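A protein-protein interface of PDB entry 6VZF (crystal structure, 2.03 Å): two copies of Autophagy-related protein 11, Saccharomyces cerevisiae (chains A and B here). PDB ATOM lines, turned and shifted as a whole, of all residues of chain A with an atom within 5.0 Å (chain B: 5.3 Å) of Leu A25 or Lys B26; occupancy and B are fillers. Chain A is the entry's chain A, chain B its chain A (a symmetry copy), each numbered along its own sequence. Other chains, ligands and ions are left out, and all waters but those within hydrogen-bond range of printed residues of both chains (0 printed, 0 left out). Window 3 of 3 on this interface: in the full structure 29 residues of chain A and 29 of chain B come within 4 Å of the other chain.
The side-chain amide oxygen (OD1) of Asn B29 sits close to the backbone carbonyl oxygen (O) of Leu A25 (3.5 Å).
The side-chain amide oxygen of Asn A29 sits close to the backbone carbonyl oxygen of Leu B25, at 3.5 Å.
OD1 of Asn A29 lies close to OD1 of Asn B29 (2.5 Å).
O of Lys A26 lies close to OD1 of Asn A30, 3.1 Å away.
The side-chain amide oxygen (OD1) of Asn B30 lies close to the backbone carbonyl oxygen (O) of Lys B26, at 3.1 Å.
N of Lys B26 touches CD2 of Leu A25, 3.8 Å away.
Lys A26 touches Leu B25.
ND2 of Asn B29 touches CB of Glu A28, at 3.4 Å.
Asn A29 touches Glu B28.
Gln A21 touches none of the printed residues of chain B.
Leu A25 touches two residues of chain B.
Of the printed residues of chain B, Lys A26 touches Leu B25.
Gln B21 touches none of the printed residues of chain A.
Of the printed residues of chain A, Leu B25 touches Lys A26 and Asn A29.
Of chain A, only Leu A25 comes within 4 Å of Lys B26.
Printed residues of chain A within 4 Å of Glu B28: Asn A29 (3.4 Å).
Of the printed residues of chain A, Asn B29 touches Leu A25, Glu A28 and Asn A29.
Printed residues of chain B that touch a printed residue of chain A: Leu B25, Lys B26, Glu B28 and Asn B29.
Hydrophobic or aromatic side chains of chain B within 4 Å of the printed part of chain A: Leu B25.
Hydrophobic or aromatic side chains of chain A that line the printed part of chain B: Leu A25.
Along chain A the printed residues that touch a printed residue of chain B span positions 25 to 29.
Among the printed residues, no Asp or Glu carboxylate lies within 4 Å of a Lys or Arg side-chain nitrogen of the other chain.
Leu A25 touches Lys B26, and with the chains exchanged Lys A26 touches Leu B25.
Leu A25 touches Asn B29, and with the chains exchanged Asn A29 touches Leu B25.
Glu A28 touches Asn B29, and with the chains exchanged Asn A29 touches Glu B28.
Asn A29 touches its own counterpart, Asn B29.
Positions printed for both chains: 21, 22, 23, 24, 25, 26, 27, 28, 29 and 30.
Of the 7 pairs that touch across the chains among the printed residues, 7 have their exchanged pair printed and touching as well.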
ATOM      1  N   GLN A  21       4.335   1.464   0.165  1.00  0.00           N
ATOM      2  CA  GLN A  21       4.399   0.004   0.445  1.00  0.00           C
ATOM      3  C   GLN A  21       3.140  -0.417   1.207  1.00  0.00           C
ATOM      4  O   GLN A  21       2.497  -1.400   0.785  1.00  0.00           O
ATOM      5  CB  GLN A  21       5.646  -0.352   1.263  1.00  0.00           C
ATOM      6  CG  GLN A  21       6.955   0.064   0.606  1.00  0.00           C
ATOM      7  CD  GLN A  21       6.847   0.184  -0.898  1.00  0.00           C
ATOM      8  OE1 GLN A  21       6.765  -0.809  -1.616  1.00  0.00           O
ATOM      9  NE2 GLN A  21       6.837   1.415  -1.394  1.00  0.00           N
ATOM     10  N   LEU A  22       2.806   0.306   2.275  1.00  0.00           N
ATOM     11  CA  LEU A  22       1.628   0.013   3.126  1.00  0.00           C
ATOM     12  C   LEU A  22       0.330   0.214   2.323  1.00  0.00           C
ATOM     13  O   LEU A  22      -0.683  -0.419   2.689  1.00  0.00           O
ATOM     14  CB  LEU A  22       1.682   0.900   4.369  1.00  0.00           C
ATOM     15  CG  LEU A  22       0.611   0.616   5.417  1.00  0.00           C
ATOM     16  CD1 LEU A  22       1.204   0.671   6.817  1.00  0.00           C
ATOM     17  CD2 LEU A  22      -0.568   1.579   5.280  1.00  0.00           C
ATOM     18  N   GLN A  23       0.343   1.050   1.277  1.00  0.00           N
ATOM     19  CA  GLN A  23      -0.764   1.139   0.284  1.00  0.00           C
ATOM     20  C   GLN A  23      -0.845  -0.192  -0.483  1.00  0.00           C
ATOM     21  O   GLN A  23      -1.926  -0.824  -0.442  1.00  0.00           O
ATOM     22  CB  GLN A  23      -0.561   2.312  -0.681  1.00  0.00           C
ATOM     23  CG  GLN A  23      -1.729   2.549  -1.635  1.00  0.00           C
ATOM     24  CD  GLN A  23      -1.307   3.086  -2.984  1.00  0.00           C
ATOM     25  OE1 GLN A  23      -0.123   3.216  -3.300  1.00  0.00           O
ATOM     26  NE2 GLN A  23      -2.292   3.396  -3.810  1.00  0.00           N
ATOM     27  N   LEU A  24       0.260  -0.589  -1.131  1.00  0.00           N
ATOM     28  CA  LEU A  24       0.397  -1.815  -1.969  1.00  0.00           C
ATOM     29  C   LEU A  24       0.029  -3.074  -1.169  1.00  0.00           C
ATOM     30  O   LEU A  24      -0.507  -4.016  -1.784  1.00  0.00           O
ATOM     31  CB  LEU A  24       1.836  -1.931  -2.482  1.00  0.00           C
ATOM     32  CG  LEU A  24       2.314  -0.837  -3.437  1.00  0.00           C
ATOM     33  CD1 LEU A  24       3.678  -1.198  -4.008  1.00  0.00           C
ATOM     34  CD2 LEU A  24       1.313  -0.585  -4.558  1.00  0.00           C
ATOM     35  N   LEU A  25       0.329  -3.105   0.132  1.00  0.00           N
ATOM     36  CA  LEU A  25       0.150  -4.305   0.985  1.00  0.00           C
ATOM     37  C   LEU A  25      -1.285  -4.405   1.475  1.00  0.00           C
ATOM     38  O   LEU A  25      -1.763  -5.553   1.619  1.00  0.00           O
ATOM     39  CB  LEU A  25       1.095  -4.279   2.182  1.00  0.00           C
ATOM     40  CG  LEU A  25       2.174  -5.350   2.123  1.00  0.00           C
ATOM     41  CD1 LEU A  25       3.142  -5.061   0.986  1.00  0.00           C
ATOM     42  CD2 LEU A  25       2.880  -5.462   3.459  1.00  0.00           C
ATOM     43  N   LYS A  26      -1.906  -3.269   1.785  1.00  0.00           N
ATOM     44  CA  LYS A  26      -3.331  -3.210   2.196  1.00  0.00           C
ATOM     45  C   LYS A  26      -4.169  -3.676   1.000  1.00  0.00           C
ATOM     46  O   LYS A  26      -5.204  -4.333   1.228  1.00  0.00           O
ATOM     47  CB  LYS A  26      -3.708  -1.797   2.647  1.00  0.00           C
ATOM     48  CG  LYS A  26      -5.081  -1.657   3.287  1.00  0.00           C
ATOM     49  CD  LYS A  26      -5.512  -0.217   3.494  1.00  0.00           C
ATOM     50  CE  LYS A  26      -6.981  -0.092   3.842  1.00  0.00           C
ATOM     51  NZ  LYS A  26      -7.380   1.320   4.051  1.00  0.00           N
ATOM     52  N   GLU A  27      -3.702  -3.331  -0.205  1.00  0.00           N
ATOM     53  CA  GLU A  27      -4.259  -3.704  -1.531  1.00  0.00           C
ATOM     54  C   GLU A  27      -4.158  -5.227  -1.723  1.00  0.00           C
ATOM     55  O   GLU A  27      -5.198  -5.847  -2.014  1.00  0.00           O
ATOM     56  CB  GLU A  27      -3.504  -2.970  -2.647  1.00  0.00           C
ATOM     57  CG  GLU A  27      -3.927  -1.519  -2.856  1.00  0.00           C
ATOM     58  CD  GLU A  27      -3.140  -0.757  -3.919  1.00  0.00           C
ATOM     59  OE1 GLU A  27      -1.895  -0.700  -3.826  1.00  0.00           O
ATOM     60  OE2 GLU A  27      -3.771  -0.215  -4.843  1.00  0.00           O
ATOM     61  N   GLU A  28      -2.952  -5.792  -1.598  1.00  0.00           N
ATOM     62  CA  GLU A  28      -2.696  -7.251  -1.673  1.00  0.00           C
ATOM     63  C   GLU A  28      -3.629  -7.971  -0.700  1.00  0.00           C
ATOM     64  O   GLU A  28      -4.461  -8.762  -1.183  1.00  0.00           O
ATOM     65  CB  GLU A  28      -1.251  -7.615  -1.352  1.00  0.00           C
ATOM     66  CG  GLU A  28      -0.378  -7.674  -2.587  1.00  0.00           C
ATOM     67  CD  GLU A  28      -1.080  -8.263  -3.800  1.00  0.00           C
ATOM     68  OE1 GLU A  28      -1.514  -9.437  -3.735  1.00  0.00           O
ATOM     69  OE2 GLU A  28      -1.236  -7.529  -4.793  1.00  0.00           O
ATOM     70  N   ASN A  29      -3.514  -7.672   0.598  1.00  0.00           N
ATOM     71  CA  ASN A  29      -4.322  -8.291   1.678  1.00  0.00           C
ATOM     72  C   ASN A  29      -5.798  -8.334   1.277  1.00  0.00           C
ATOM     73  O   ASN A  29      -6.482  -9.300   1.687  1.00  0.00           O
ATOM     74  CB  ASN A  29      -4.213  -7.569   3.018  1.00  0.00           C
ATOM     75  CG  ASN A  29      -3.508  -8.377   4.089  1.00  0.00           C
ATOM     76  OD1 ASN A  29      -2.333  -8.752   3.945  1.00  0.00           O
ATOM     77  ND2 ASN A  29      -4.226  -8.640   5.172  1.00  0.00           N
ATOM     78  N   ASN A  30      -6.276  -7.305   0.570  1.00  0.00           N
ATOM     79  CA  ASN A  30      -7.690  -7.185   0.135  1.00  0.00           C
ATOM     80  C   ASN A  30      -7.973  -8.169  -1.003  1.00  0.00           C
ATOM     81  O   ASN A  30      -9.049  -8.781  -0.945  1.00  0.00           O
ATOM     82  CB  ASN A  30      -8.054  -5.786  -0.369  1.00  0.00           C
ATOM     83  CG  ASN A  30      -8.124  -4.745   0.726  1.00  0.00           C
ATOM     84  OD1 ASN A  30      -8.163  -5.078   1.908  1.00  0.00           O
ATOM     85  ND2 ASN A  30      -8.146  -3.480   0.335  1.00  0.00           N
ATOM     86  N   GLN B  21       2.478  -1.844  12.096  1.00  0.00           N
ATOM     87  CA  GLN B  21       1.375  -2.181  11.157  1.00  0.00           C
ATOM     88  C   GLN B  21       1.949  -2.944   9.960  1.00  0.00           C
ATOM     89  O   GLN B  21       1.403  -4.015   9.627  1.00  0.00           O
ATOM     90  CB  GLN B  21       0.653  -0.919  10.672  1.00  0.00           C
ATOM     91  CG  GLN B  21       0.078  -0.066  11.794  1.00  0.00           C
ATOM     92  CD  GLN B  21      -0.204  -0.860  13.051  1.00  0.00           C
ATOM     93  OE1 GLN B  21      -1.149  -1.642  13.117  1.00  0.00           O
ATOM     94  NE2 GLN B  21       0.627  -0.672  14.069  1.00  0.00           N
ATOM     95  N   LEU B  22       3.010  -2.412   9.353  1.00  0.00           N
ATOM     96  CA  LEU B  22       3.666  -3.019   8.171  1.00  0.00           C
ATOM     97  C   LEU B  22       4.298  -4.370   8.551  1.00  0.00           C
ATOM     98  O   LEU B  22       4.458  -5.214   7.643  1.00  0.00           O
ATOM     99  CB  LEU B  22       4.694  -2.035   7.615  1.00  0.00           C
ATOM    100  CG  LEU B  22       5.357  -2.458   6.307  1.00  0.00           C
ATOM    101  CD1 LEU B  22       5.483  -1.271   5.364  1.00  0.00           C
ATOM    102  CD2 LEU B  22       6.718  -3.107   6.560  1.00  0.00           C
ATOM    103  N   GLN B  23       4.647  -4.581   9.827  1.00  0.00           N
ATOM    104  CA  GLN B  23       5.033  -5.917  10.362  1.00  0.00           C
ATOM    105  C   GLN B  23       3.807  -6.845  10.300  1.00  0.00           C
ATOM    106  O   GLN B  23       3.909  -7.903   9.638  1.00  0.00           O
ATOM    107  CB  GLN B  23       5.567  -5.817  11.795  1.00  0.00           C
ATOM    108  CG  GLN B  23       6.114  -7.128  12.354  1.00  0.00           C
ATOM    109  CD  GLN B  23       5.916  -7.276  13.846  1.00  0.00           C
ATOM    110  OE1 GLN B  23       5.282  -6.455  14.511  1.00  0.00           O
ATOM    111  NE2 GLN B  23       6.458  -8.353  14.391  1.00  0.00           N
ATOM    112  N   LEU B  24       2.706  -6.442  10.950  1.00  0.00           N
ATOM    113  CA  LEU B  24       1.423  -7.195  11.061  1.00  0.00           C
ATOM    114  C   LEU B  24       0.863  -7.539   9.671  1.00  0.00           C
ATOM    115  O   LEU B  24       0.235  -8.608   9.548  1.00  0.00           O
ATOM    116  CB  LEU B  24       0.400  -6.360  11.838  1.00  0.00           C
ATOM    117  CG  LEU B  24       0.725  -6.066  13.302  1.00  0.00           C
ATOM    118  CD1 LEU B  24      -0.467  -5.408  13.982  1.00  0.00           C
ATOM    119  CD2 LEU B  24       1.144  -7.324  14.054  1.00  0.00           C
ATOM    120  N   LEU B  25       1.052  -6.663   8.681  1.00  0.00           N
ATOM    121  CA  LEU B  25       0.451  -6.811   7.333  1.00  0.00           C
ATOM    122  C   LEU B  25       1.295  -7.732   6.467  1.00  0.00           C
ATOM    123  O   LEU B  25       0.694  -8.451   5.638  1.00  0.00           O
ATOM    124  CB  LEU B  25       0.303  -5.459   6.642  1.00  0.00           C
ATOM    125  CG  LEU B  25      -1.144  -5.026   6.467  1.00  0.00           C
ATOM    126  CD1 LEU B  25      -1.772  -4.728   7.820  1.00  0.00           C
ATOM    127  CD2 LEU B  25      -1.230  -3.843   5.525  1.00  0.00           C
ATOM    128  N   LYS B  26       2.618  -7.656   6.603  1.00  0.00           N
ATOM    129  CA  LYS B  26       3.559  -8.552   5.885  1.00  0.00           C
ATOM    130  C   LYS B  26       3.302  -9.977   6.386  1.00  0.00           C
ATOM    131  O   LYS B  26       3.413 -10.915   5.572  1.00  0.00           O
ATOM    132  CB  LYS B  26       5.007  -8.113   6.113  1.00  0.00           C
ATOM    133  CG  LYS B  26       6.050  -8.825   5.264  1.00  0.00           C
ATOM    134  CD  LYS B  26       7.479  -8.540   5.690  1.00  0.00           C
ATOM    135  CE  LYS B  26       8.477  -9.479   5.044  1.00  0.00           C
ATOM    136  NZ  LYS B  26       9.866  -9.178   5.463  1.00  0.00           N
ATOM    137  N   GLU B  27       2.971 -10.088   7.677  1.00  0.00           N
ATOM    138  CA  GLU B  27       2.597 -11.324   8.412  1.00  0.00           C
ATOM    139  C   GLU B  27       1.288 -11.890   7.837  1.00  0.00           C
ATOM    140  O   GLU B  27       1.281 -13.077   7.464  1.00  0.00           O
ATOM    141  CB  GLU B  27       2.441 -11.022   9.908  1.00  0.00           C
ATOM    142  CG  GLU B  27       3.753 -10.937  10.682  1.00  0.00           C
ATOM    143  CD  GLU B  27       3.618 -10.574  12.158  1.00  0.00           C
ATOM    144  OE1 GLU B  27       3.012  -9.526  12.471  1.00  0.00           O
ATOM    145  OE2 GLU B  27       4.121 -11.337  13.001  1.00  0.00           O
ATOM    146  N   GLU B  28       0.222 -11.081   7.801  1.00  0.00           N
ATOM    147  CA  GLU B  28      -1.088 -11.444   7.207  1.00  0.00           C
ATOM    148  C   GLU B  28      -0.865 -11.951   5.783  1.00  0.00           C
ATOM    149  O   GLU B  28      -1.175 -13.134   5.542  1.00  0.00           O
ATOM    150  CB  GLU B  28      -2.068 -10.277   7.181  1.00  0.00           C
ATOM    151  CG  GLU B  28      -2.947 -10.228   8.412  1.00  0.00           C
ATOM    152  CD  GLU B  28      -3.379 -11.599   8.905  1.00  0.00           C
ATOM    153  OE1 GLU B  28      -4.049 -12.333   8.140  1.00  0.00           O
ATOM    154  OE2 GLU B  28      -3.004 -11.954  10.038  1.00  0.00           O
ATOM    155  N   ASN B  29      -0.317 -11.104   4.906  1.00  0.00           N
ATOM    156  CA  ASN B  29      -0.052 -11.424   3.481  1.00  0.00           C
ATOM    157  C   ASN B  29       0.601 -12.802   3.360  1.00  0.00           C
ATOM    158  O   ASN B  29       0.331 -13.485   2.345  1.00  0.00           O
ATOM    159  CB  ASN B  29       0.844 -10.408   2.779  1.00  0.00           C
ATOM    160  CG  ASN B  29       0.135  -9.609   1.705  1.00  0.00           C
ATOM    161  OD1 ASN B  29      -0.842  -8.891   1.975  1.00  0.00           O
ATOM    162  ND2 ASN B  29       0.631  -9.728   0.482  1.00  0.00           N
ATOM    163  N   ASN B  30       1.467 -13.160   4.314  1.00  0.00           N
ATOM    164  CA  ASN B  30       2.205 -14.448   4.320  1.00  0.00           C
ATOM    165  C   ASN B  30       1.255 -15.595   4.675  1.00  0.00           C
ATOM    166  O   ASN B  30       1.376 -16.633   4.010  1.00  0.00           O
ATOM    167  CB  ASN B  30       3.360 -14.482   5.324  1.00  0.00           C
ATOM    168  CG  ASN B  30       4.534 -13.615   4.931  1.00  0.00           C
ATOM    169  OD1 ASN B  30       4.635 -13.175   3.788  1.00  0.00           O
ATOM    170  ND2 ASN B  30       5.429 -13.371   5.876  1.00  0.00           N
